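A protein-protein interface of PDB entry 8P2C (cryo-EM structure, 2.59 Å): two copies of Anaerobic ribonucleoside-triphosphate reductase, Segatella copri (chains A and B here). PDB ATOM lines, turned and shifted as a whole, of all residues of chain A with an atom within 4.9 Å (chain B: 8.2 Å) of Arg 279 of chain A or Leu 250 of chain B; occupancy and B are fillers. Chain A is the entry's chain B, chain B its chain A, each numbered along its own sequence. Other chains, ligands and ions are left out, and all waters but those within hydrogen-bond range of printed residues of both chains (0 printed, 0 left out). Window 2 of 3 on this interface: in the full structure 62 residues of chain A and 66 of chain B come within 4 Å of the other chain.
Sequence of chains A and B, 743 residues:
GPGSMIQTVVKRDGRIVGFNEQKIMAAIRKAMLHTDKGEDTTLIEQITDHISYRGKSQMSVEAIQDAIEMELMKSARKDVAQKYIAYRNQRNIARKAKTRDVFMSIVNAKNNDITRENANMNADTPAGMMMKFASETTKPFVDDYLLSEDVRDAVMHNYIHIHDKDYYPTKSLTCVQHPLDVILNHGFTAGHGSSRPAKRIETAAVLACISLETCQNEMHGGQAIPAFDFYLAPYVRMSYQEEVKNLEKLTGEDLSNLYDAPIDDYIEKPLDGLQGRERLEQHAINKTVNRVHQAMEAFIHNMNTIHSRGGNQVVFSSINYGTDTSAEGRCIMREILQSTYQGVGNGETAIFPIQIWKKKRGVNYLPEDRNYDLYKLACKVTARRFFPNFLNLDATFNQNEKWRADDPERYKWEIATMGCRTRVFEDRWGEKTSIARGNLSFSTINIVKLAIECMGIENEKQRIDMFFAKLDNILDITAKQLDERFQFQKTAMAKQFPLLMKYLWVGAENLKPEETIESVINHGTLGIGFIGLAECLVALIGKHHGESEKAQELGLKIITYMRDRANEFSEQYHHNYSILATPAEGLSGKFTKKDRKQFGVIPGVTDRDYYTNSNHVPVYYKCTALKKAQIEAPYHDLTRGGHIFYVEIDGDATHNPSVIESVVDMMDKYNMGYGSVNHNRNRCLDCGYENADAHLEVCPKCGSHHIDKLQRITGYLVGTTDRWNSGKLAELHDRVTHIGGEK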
ATOM      1  N   LEU A 247      -2.448  -8.422  17.876  1.00  0.00           N
ATOM      2  CA  LEU A 247      -2.076  -7.218  17.142  1.00  0.00           C
ATOM      3  C   LEU A 247      -2.552  -5.963  17.860  1.00  0.00           C
ATOM      4  O   LEU A 247      -1.833  -4.958  17.907  1.00  0.00           O
ATOM      5  CB  LEU A 247      -2.653  -7.279  15.730  1.00  0.00           C
ATOM      6  CG  LEU A 247      -1.831  -6.608  14.639  1.00  0.00           C
ATOM      7  CD1 LEU A 247      -0.370  -6.961  14.800  1.00  0.00           C
ATOM      8  CD2 LEU A 247      -2.336  -7.048  13.284  1.00  0.00           C
ATOM      9  N   LEU A 271       2.542  -6.421   1.968  1.00  0.00           N
ATOM     10  CA  LEU A 271       2.142  -5.431   2.957  1.00  0.00           C
ATOM     11  C   LEU A 271       2.486  -4.000   2.570  1.00  0.00           C
ATOM     12  O   LEU A 271       1.847  -3.071   3.076  1.00  0.00           O
ATOM     13  CB  LEU A 271       2.787  -5.756   4.309  1.00  0.00           C
ATOM     14  CG  LEU A 271       2.122  -5.181   5.557  1.00  0.00           C
ATOM     15  CD1 LEU A 271       0.671  -5.613   5.628  1.00  0.00           C
ATOM     16  CD2 LEU A 271       2.875  -5.616   6.801  1.00  0.00           C
ATOM     17  N   ASP A 272       3.469  -3.793   1.696  1.00  0.00           N
ATOM     18  CA  ASP A 272       3.880  -2.441   1.340  1.00  0.00           C
ATOM     19  C   ASP A 272       2.819  -1.764   0.481  1.00  0.00           C
ATOM     20  O   ASP A 272       2.333  -2.339  -0.498  1.00  0.00           O
ATOM     21  CB  ASP A 272       5.215  -2.472   0.600  1.00  0.00           C
ATOM     22  CG  ASP A 272       6.344  -3.002   1.460  1.00  0.00           C
ATOM     23  OD1 ASP A 272       6.300  -2.798   2.692  1.00  0.00           O
ATOM     24  OD2 ASP A 272       7.275  -3.621   0.905  1.00  0.00           O
ATOM     25  N   LEU A 274       0.304   0.554   2.140  1.00  0.00           N
ATOM     26  CA  LEU A 274      -0.761   1.102   2.967  1.00  0.00           C
ATOM     27  C   LEU A 274      -0.280   1.215   4.405  1.00  0.00           C
ATOM     28  O   LEU A 274       0.710   0.596   4.802  1.00  0.00           O
ATOM     29  CB  LEU A 274      -2.038   0.254   2.887  1.00  0.00           C
ATOM     30  CG  LEU A 274      -1.896  -1.218   2.500  1.00  0.00           C
ATOM     31  CD1 LEU A 274      -1.239  -2.025   3.609  1.00  0.00           C
ATOM     32  CD2 LEU A 274      -3.249  -1.798   2.138  1.00  0.00           C
ATOM     33  N   GLN A 275      -0.999   2.024   5.178  1.00  0.00           N
ATOM     34  CA  GLN A 275      -0.642   2.292   6.563  1.00  0.00           C
ATOM     35  C   GLN A 275      -1.922   2.455   7.371  1.00  0.00           C
ATOM     36  O   GLN A 275      -2.992   2.727   6.825  1.00  0.00           O
ATOM     37  CB  GLN A 275       0.242   3.539   6.675  1.00  0.00           C
ATOM     38  CG  GLN A 275       0.938   3.715   8.015  1.00  0.00           C
ATOM     39  CD  GLN A 275       1.719   5.013   8.096  1.00  0.00           C
ATOM     40  OE1 GLN A 275       2.355   5.305   9.110  1.00  0.00           O
ATOM     41  NE2 GLN A 275       1.674   5.800   7.028  1.00  0.00           N
ATOM     42  N   GLY A 276      -1.801   2.266   8.682  1.00  0.00           N
ATOM     43  CA  GLY A 276      -2.918   2.481   9.577  1.00  0.00           C
ATOM     44  C   GLY A 276      -3.757   1.249   9.842  1.00  0.00           C
ATOM     45  O   GLY A 276      -3.231   0.137   9.947  1.00  0.00           O
ATOM     46  N   ARG A 277      -5.072   1.444   9.957  1.00  0.00           N
ATOM     47  CA  ARG A 277      -5.963   0.336  10.283  1.00  0.00           C
ATOM     48  C   ARG A 277      -6.022  -0.685   9.153  1.00  0.00           C
ATOM     49  O   ARG A 277      -6.138  -1.890   9.404  1.00  0.00           O
ATOM     50  CB  ARG A 277      -7.357   0.867  10.604  1.00  0.00           C
ATOM     51  CG  ARG A 277      -8.431  -0.196  10.691  1.00  0.00           C
ATOM     52  CD  ARG A 277      -9.769   0.413  11.062  1.00  0.00           C
ATOM     53  NE  ARG A 277      -9.893   0.629  12.497  1.00  0.00           N
ATOM     54  CZ  ARG A 277     -10.712  -0.052  13.287  1.00  0.00           C
ATOM     55  NH1 ARG A 277     -11.515  -0.987  12.806  1.00  0.00           N
ATOM     56  NH2 ARG A 277     -10.730   0.217  14.588  1.00  0.00           N
ATOM     57  N   GLU A 278      -5.941  -0.226   7.904  1.00  0.00           N
ATOM     58  CA  GLU A 278      -5.996  -1.153   6.778  1.00  0.00           C
ATOM     59  C   GLU A 278      -4.796  -2.091   6.770  1.00  0.00           C
ATOM     60  O   GLU A 278      -4.931  -3.277   6.448  1.00  0.00           O
ATOM     61  CB  GLU A 278      -6.085  -0.383   5.462  1.00  0.00           C
ATOM     62  CG  GLU A 278      -7.506  -0.114   5.001  1.00  0.00           C
ATOM     63  CD  GLU A 278      -8.231  -1.380   4.585  1.00  0.00           C
ATOM     64  OE1 GLU A 278      -7.558  -2.403   4.338  1.00  0.00           O
ATOM     65  OE2 GLU A 278      -9.477  -1.354   4.505  1.00  0.00           O
ATOM     66  N   ARG A 279      -3.612  -1.578   7.106  1.00  0.00           N
ATOM     67  CA  ARG A 279      -2.424  -2.426   7.115  1.00  0.00           C
ATOM     68  C   ARG A 279      -2.519  -3.512   8.180  1.00  0.00           C
ATOM     69  O   ARG A 279      -2.193  -4.675   7.916  1.00  0.00           O
ATOM     70  CB  ARG A 279      -1.170  -1.581   7.326  1.00  0.00           C
ATOM     71  CG  ARG A 279      -0.058  -2.333   8.029  1.00  0.00           C
ATOM     72  CD  ARG A 279       1.238  -1.558   8.052  1.00  0.00           C
ATOM     73  NE  ARG A 279       1.991  -1.723   6.817  1.00  0.00           N
ATOM     74  CZ  ARG A 279       3.288  -1.479   6.701  1.00  0.00           C
ATOM     75  NH1 ARG A 279       4.009  -1.071   7.731  1.00  0.00           N
ATOM     76  NH2 ARG A 279       3.877  -1.655   5.522  1.00  0.00           N
ATOM     77  N   LEU A 280      -2.975  -3.163   9.383  1.00  0.00           N
ATOM     78  CA  LEU A 280      -3.045  -4.132  10.467  1.00  0.00           C
ATOM     79  C   LEU A 280      -4.237  -5.074  10.348  1.00  0.00           C
ATOM     80  O   LEU A 280      -4.539  -5.789  11.308  1.00  0.00           O
ATOM     81  CB  LEU A 280      -3.063  -3.419  11.823  1.00  0.00           C
ATOM     82  CG  LEU A 280      -4.033  -2.282  12.136  1.00  0.00           C
ATOM     83  CD1 LEU A 280      -5.441  -2.784  12.404  1.00  0.00           C
ATOM     84  CD2 LEU A 280      -3.515  -1.498  13.328  1.00  0.00           C
ATOM     85  N   GLU A 281      -4.924  -5.083   9.209  1.00  0.00           N
ATOM     86  CA  GLU A 281      -5.876  -6.137   8.895  1.00  0.00           C
ATOM     87  C   GLU A 281      -5.281  -7.195   7.978  1.00  0.00           C
ATOM     88  O   GLU A 281      -5.831  -8.297   7.886  1.00  0.00           O
ATOM     89  CB  GLU A 281      -7.134  -5.545   8.248  1.00  0.00           C
ATOM     90  CG  GLU A 281      -8.267  -6.539   8.062  1.00  0.00           C
ATOM     91  CD  GLU A 281      -9.445  -5.949   7.319  1.00  0.00           C
ATOM     92  OE1 GLU A 281      -9.430  -4.728   7.055  1.00  0.00           O
ATOM     93  OE2 GLU A 281     -10.385  -6.705   7.000  1.00  0.00           O
ATOM     94  N   GLN A 282      -4.162  -6.901   7.324  1.00  0.00           N
ATOM     95  CA  GLN A 282      -3.537  -7.834   6.397  1.00  0.00           C
ATOM     96  C   GLN A 282      -2.440  -8.662   7.045  1.00  0.00           C
ATOM     97  O   GLN A 282      -2.170  -9.781   6.598  1.00  0.00           O
ATOM     98  CB  GLN A 282      -2.966  -7.082   5.193  1.00  0.00           C
ATOM     99  CG  GLN A 282      -3.078  -7.844   3.886  1.00  0.00           C
ATOM    100  CD  GLN A 282      -4.516  -8.027   3.441  1.00  0.00           C
ATOM    101  OE1 GLN A 282      -5.403  -7.275   3.842  1.00  0.00           O
ATOM    102  NE2 GLN A 282      -4.755  -9.032   2.607  1.00  0.00           N
ATOM    103  N   HIS A 283      -1.791  -8.132   8.081  1.00  0.00           N
ATOM    104  CA  HIS A 283      -0.836  -8.926   8.846  1.00  0.00           C
ATOM    105  C   HIS A 283      -1.522 -10.124   9.490  1.00  0.00           C
ATOM    106  O   HIS A 283      -0.980 -11.239   9.497  1.00  0.00           O
ATOM    107  CB  HIS A 283      -0.177  -8.050   9.908  1.00  0.00           C
ATOM    108  CG  HIS A 283       1.185  -8.510  10.317  1.00  0.00           C
ATOM    109  ND1 HIS A 283       1.635  -8.435  11.617  1.00  0.00           N
ATOM    110  CD2 HIS A 283       2.202  -9.035   9.596  1.00  0.00           C
ATOM    111  CE1 HIS A 283       2.868  -8.903  11.681  1.00  0.00           C
ATOM    112  NE2 HIS A 283       3.236  -9.273  10.469  1.00  0.00           N
ATOM    113  N   VAL B 244      10.721 -11.445  16.055  1.00  0.00           N
ATOM    114  CA  VAL B 244      11.300 -10.135  15.767  1.00  0.00           C
ATOM    115  C   VAL B 244      11.165  -9.796  14.289  1.00  0.00           C
ATOM    116  O   VAL B 244      10.816  -8.662  13.931  1.00  0.00           O
ATOM    117  CB  VAL B 244      12.768 -10.088  16.231  1.00  0.00           C
ATOM    118  CG1 VAL B 244      13.414  -8.783  15.809  1.00  0.00           C
ATOM    119  CG2 VAL B 244      12.849 -10.247  17.735  1.00  0.00           C
ATOM    120  N   LYS B 245      11.424 -10.764  13.406  1.00  0.00           N
ATOM    121  CA  LYS B 245      11.319 -10.517  11.973  1.00  0.00           C
ATOM    122  C   LYS B 245       9.889 -10.270  11.520  1.00  0.00           C
ATOM    123  O   LYS B 245       9.683  -9.558  10.532  1.00  0.00           O
ATOM    124  CB  LYS B 245      11.907 -11.688  11.186  1.00  0.00           C
ATOM    125  CG  LYS B 245      13.412 -11.816  11.305  1.00  0.00           C
ATOM    126  CD  LYS B 245      13.931 -12.952  10.447  1.00  0.00           C
ATOM    127  CE  LYS B 245      15.441 -13.074  10.549  1.00  0.00           C
ATOM    128  NZ  LYS B 245      15.886 -13.325  11.947  1.00  0.00           N
ATOM    129  N   ASN B 246       8.901 -10.837  12.206  1.00  0.00           N
ATOM    130  CA  ASN B 246       7.521 -10.501  11.887  1.00  0.00           C
ATOM    131  C   ASN B 246       7.135  -9.136  12.434  1.00  0.00           C
ATOM    132  O   ASN B 246       6.289  -8.451  11.850  1.00  0.00           O
ATOM    133  CB  ASN B 246       6.568 -11.572  12.424  1.00  0.00           C
ATOM    134  CG  ASN B 246       6.097 -12.526  11.344  1.00  0.00           C
ATOM    135  OD1 ASN B 246       5.077 -12.292  10.693  1.00  0.00           O
ATOM    136  ND2 ASN B 246       6.839 -13.608  11.147  1.00  0.00           N
ATOM    137  N   LEU B 247       7.738  -8.730  13.555  1.00  0.00           N
ATOM    138  CA  LEU B 247       7.518  -7.376  14.054  1.00  0.00           C
ATOM    139  C   LEU B 247       8.084  -6.334  13.099  1.00  0.00           C
ATOM    140  O   LEU B 247       7.474  -5.279  12.890  1.00  0.00           O
ATOM    141  CB  LEU B 247       8.130  -7.216  15.441  1.00  0.00           C
ATOM    142  CG  LEU B 247       7.188  -7.592  16.577  1.00  0.00           C
ATOM    143  CD1 LEU B 247       7.851  -7.360  17.911  1.00  0.00           C
ATOM    144  CD2 LEU B 247       5.905  -6.794  16.465  1.00  0.00           C
ATOM    145  N   GLU B 248       9.254  -6.608  12.519  1.00  0.00           N
ATOM    146  CA  GLU B 248       9.878  -5.697  11.566  1.00  0.00           C
ATOM    147  C   GLU B 248       8.931  -5.341  10.425  1.00  0.00           C
ATOM    148  O   GLU B 248       8.776  -4.164  10.086  1.00  0.00           O
ATOM    149  CB  GLU B 248      11.161  -6.304  10.994  1.00  0.00           C
ATOM    150  CG  GLU B 248      12.288  -6.425  11.996  1.00  0.00           C
ATOM    151  CD  GLU B 248      13.529  -7.066  11.407  1.00  0.00           C
ATOM    152  OE1 GLU B 248      13.576  -7.252  10.173  1.00  0.00           O
ATOM    153  OE2 GLU B 248      14.457  -7.388  12.179  1.00  0.00           O
ATOM    154  N   LYS B 249       8.294  -6.352   9.838  1.00  0.00           N
ATOM    155  CA  LYS B 249       7.455  -6.168   8.659  1.00  0.00           C
ATOM    156  C   LYS B 249       6.318  -5.185   8.906  1.00  0.00           C
ATOM    157  O   LYS B 249       6.030  -4.341   8.053  1.00  0.00           O
ATOM    158  CB  LYS B 249       6.891  -7.513   8.201  1.00  0.00           C
ATOM    159  CG  LYS B 249       6.156  -7.464   6.876  1.00  0.00           C
ATOM    160  CD  LYS B 249       5.550  -8.815   6.540  1.00  0.00           C
ATOM    161  CE  LYS B 249       5.740  -9.158   5.074  1.00  0.00           C
ATOM    162  NZ  LYS B 249       5.130  -8.139   4.178  1.00  0.00           N
ATOM    163  N   LEU B 250       5.663  -5.284  10.063  1.00  0.00           N
ATOM    164  CA  LEU B 250       4.527  -4.412  10.346  1.00  0.00           C
ATOM    165  C   LEU B 250       4.984  -2.980  10.590  1.00  0.00           C
ATOM    166  O   LEU B 250       4.634  -2.063   9.839  1.00  0.00           O
ATOM    167  CB  LEU B 250       3.750  -4.940  11.552  1.00  0.00           C
ATOM    168  CG  LEU B 250       2.496  -4.155  11.931  1.00  0.00           C
ATOM    169  CD1 LEU B 250       1.431  -4.275  10.853  1.00  0.00           C
ATOM    170  CD2 LEU B 250       1.961  -4.621  13.270  1.00  0.00           C
ATOM    171  N   THR B 251       5.773  -2.771  11.643  1.00  0.00           N
ATOM    172  CA  THR B 251       6.345  -1.461  11.942  1.00  0.00           C
ATOM    173  C   THR B 251       7.747  -1.421  11.344  1.00  0.00           C
ATOM    174  O   THR B 251       8.739  -1.799  11.971  1.00  0.00           O
ATOM    175  CB  THR B 251       6.357  -1.206  13.443  1.00  0.00           C
ATOM    176  OG1 THR B 251       7.169  -2.192  14.093  1.00  0.00           O
ATOM    177  CG2 THR B 251       4.944  -1.275  14.005  1.00  0.00           C
ATOM    178  N   GLY B 252       7.819  -0.957  10.098  1.00  0.00           N
ATOM    179  CA  GLY B 252       9.060  -0.970   9.351  1.00  0.00           C
ATOM    180  C   GLY B 252      10.212  -0.297  10.067  1.00  0.00           C
ATOM    181  O   GLY B 252      10.240   0.928  10.215  1.00  0.00           O
ATOM    182  N   GLU B 253      11.171  -1.105  10.509  1.00  0.00           N
ATOM    183  CA  GLU B 253      12.355  -0.630  11.212  1.00  0.00           C
ATOM    184  C   GLU B 253      13.512  -1.554  10.853  1.00  0.00           C
ATOM    185  O   GLU B 253      13.458  -2.297   9.869  1.00  0.00           O
ATOM    186  CB  GLU B 253      12.119  -0.570  12.728  1.00  0.00           C
ATOM    187  CG  GLU B 253      11.162   0.517  13.180  1.00  0.00           C
ATOM    188  CD  GLU B 253      11.174   0.722  14.680  1.00  0.00           C
ATOM    189  OE1 GLU B 253      12.066   0.162  15.350  1.00  0.00           O
ATOM    190  OE2 GLU B 253      10.290   1.442  15.188  1.00  0.00           O
ATOM    191  N   LEU B 255      15.661  -3.403  13.662  1.00  0.00           N
ATOM    192  CA  LEU B 255      15.614  -4.484  14.648  1.00  0.00           C
ATOM    193  C   LEU B 255      16.663  -5.556  14.364  1.00  0.00           C
ATOM    194  O   LEU B 255      16.473  -6.733  14.680  1.00  0.00           O
ATOM    195  CB  LEU B 255      14.217  -5.104  14.723  1.00  0.00           C
ATOM    196  CG  LEU B 255      13.068  -4.163  15.085  1.00  0.00           C
ATOM    197  CD1 LEU B 255      11.779  -4.943  15.283  1.00  0.00           C
ATOM    198  CD2 LEU B 255      13.397  -3.350  16.324  1.00  0.00           C
ATOM    199  N   LEU B 280       8.687  -2.948  21.762  1.00  0.00           N
ATOM    200  CA  LEU B 280       8.705  -3.918  20.677  1.00  0.00           C
ATOM    201  C   LEU B 280       9.629  -5.095  20.951  1.00  0.00           C
ATOM    202  O   LEU B 280       9.540  -6.104  20.246  1.00  0.00           O
ATOM    203  CB  LEU B 280       9.115  -3.236  19.372  1.00  0.00           C
ATOM    204  CG  LEU B 280       8.077  -3.253  18.250  1.00  0.00           C
ATOM    205  CD1 LEU B 280       6.766  -2.661  18.730  1.00  0.00           C
ATOM    206  CD2 LEU B 280       8.595  -2.497  17.043  1.00  0.00           C
ATOM    207  N   HIS B 283       7.126  -7.472  23.399  1.00  0.00           N
ATOM    208  CA  HIS B 283       6.031  -8.196  22.773  1.00  0.00           C
ATOM    209  C   HIS B 283       6.517  -9.415  22.006  1.00  0.00           C
ATOM    210  O   HIS B 283       5.790 -10.412  21.918  1.00  0.00           O
ATOM    211  CB  HIS B 283       5.256  -7.271  21.835  1.00  0.00           C
ATOM    212  CG  HIS B 283       4.071  -7.918  21.193  1.00  0.00           C
ATOM    213  ND1 HIS B 283       4.055  -8.290  19.866  1.00  0.00           N
ATOM    214  CD2 HIS B 283       2.859  -8.252  21.692  1.00  0.00           C
ATOM    215  CE1 HIS B 283       2.884  -8.826  19.577  1.00  0.00           C
ATOM    216  NE2 HIS B 283       2.141  -8.817  20.667  1.00  0.00           N
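The backbone carbonyl oxygen of Asn 246 of chain B lies within hydrogen-bond range of a ring nitrogen (NE2) of His 283 of chain A. NH1 of Arg 279 of chain A sits at hydrogen-bond distance from O of Leu 250 of chain B (2.4 Å).
O of Leu 271 of chain A is in hydrogen-bond range of NH2 of Arg 279 of chain A (3.5 Å). The side-chain carboxylate of Asp 272 of chain A lies within salt-bridge range of the guanidinium group of Arg 279 of chain A (3.9 Å). The backbone carbonyl oxygen (O) of Leu 274 of chain A sits at hydrogen-bond distance from the guanidinium group (NE) of Arg 279 of chain A, 3.3 Å away.
Among the printed residues, pairs that only touch across the chains: Leu 247 of chain A with Leu 250 of chain B (3.6 Å), Leu 271 of chain A with Lys 249 of chain B (3.3 Å) and Arg 279 of chain A with Lys 249 of chain B (3.9 Å).
Printed residues of chain B within 4 Å of Leu 247 of chain A: Leu 250 (3.6 Å). Of the printed residues of chain B, His 283 of chain A touches Asn 246 (3.5 Å). Printed residues of chain A within 4 Å of Asn 246 of chain B: His 283. Printed residues of chain A within 4 Å of Lys 249 of chain B: Leu 271 (3.3 Å) and Arg 279 (3.9 Å). Leu 250 of chain B touches two residues of chain A. The nearest residue of chain B that does not touch Arg 279 of chain A is Gly 252 of chain B (4.5 Å). The nearest residue of chain A that does not touch Leu 250 of chain B is His 283 of chain A (4.1 Å). The nearest printed residue of chain B that does not touch Leu 271 of chain A is Leu 250 of chain B (4.1 Å).
Of the 13 printed residues of chain B, 3 touch a printed residue of chain A. Hydrophobic or aromatic side chains of chain B within 4 Å of the printed part of chain A: Leu 250. Of the 13 printed residues of chain A, 4 touch a printed residue of chain B. Hydrophobic or aromatic side chains of chain A that line the printed part of chain B: Leu 247, Leu 271 and His 283. Among the printed residues, 5 pairs touch across the chains.
3 positions are printed for both chains. Of the 5 pairs that touch across the chains among the printed residues, none has its exchanged pair printed and touching as well.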
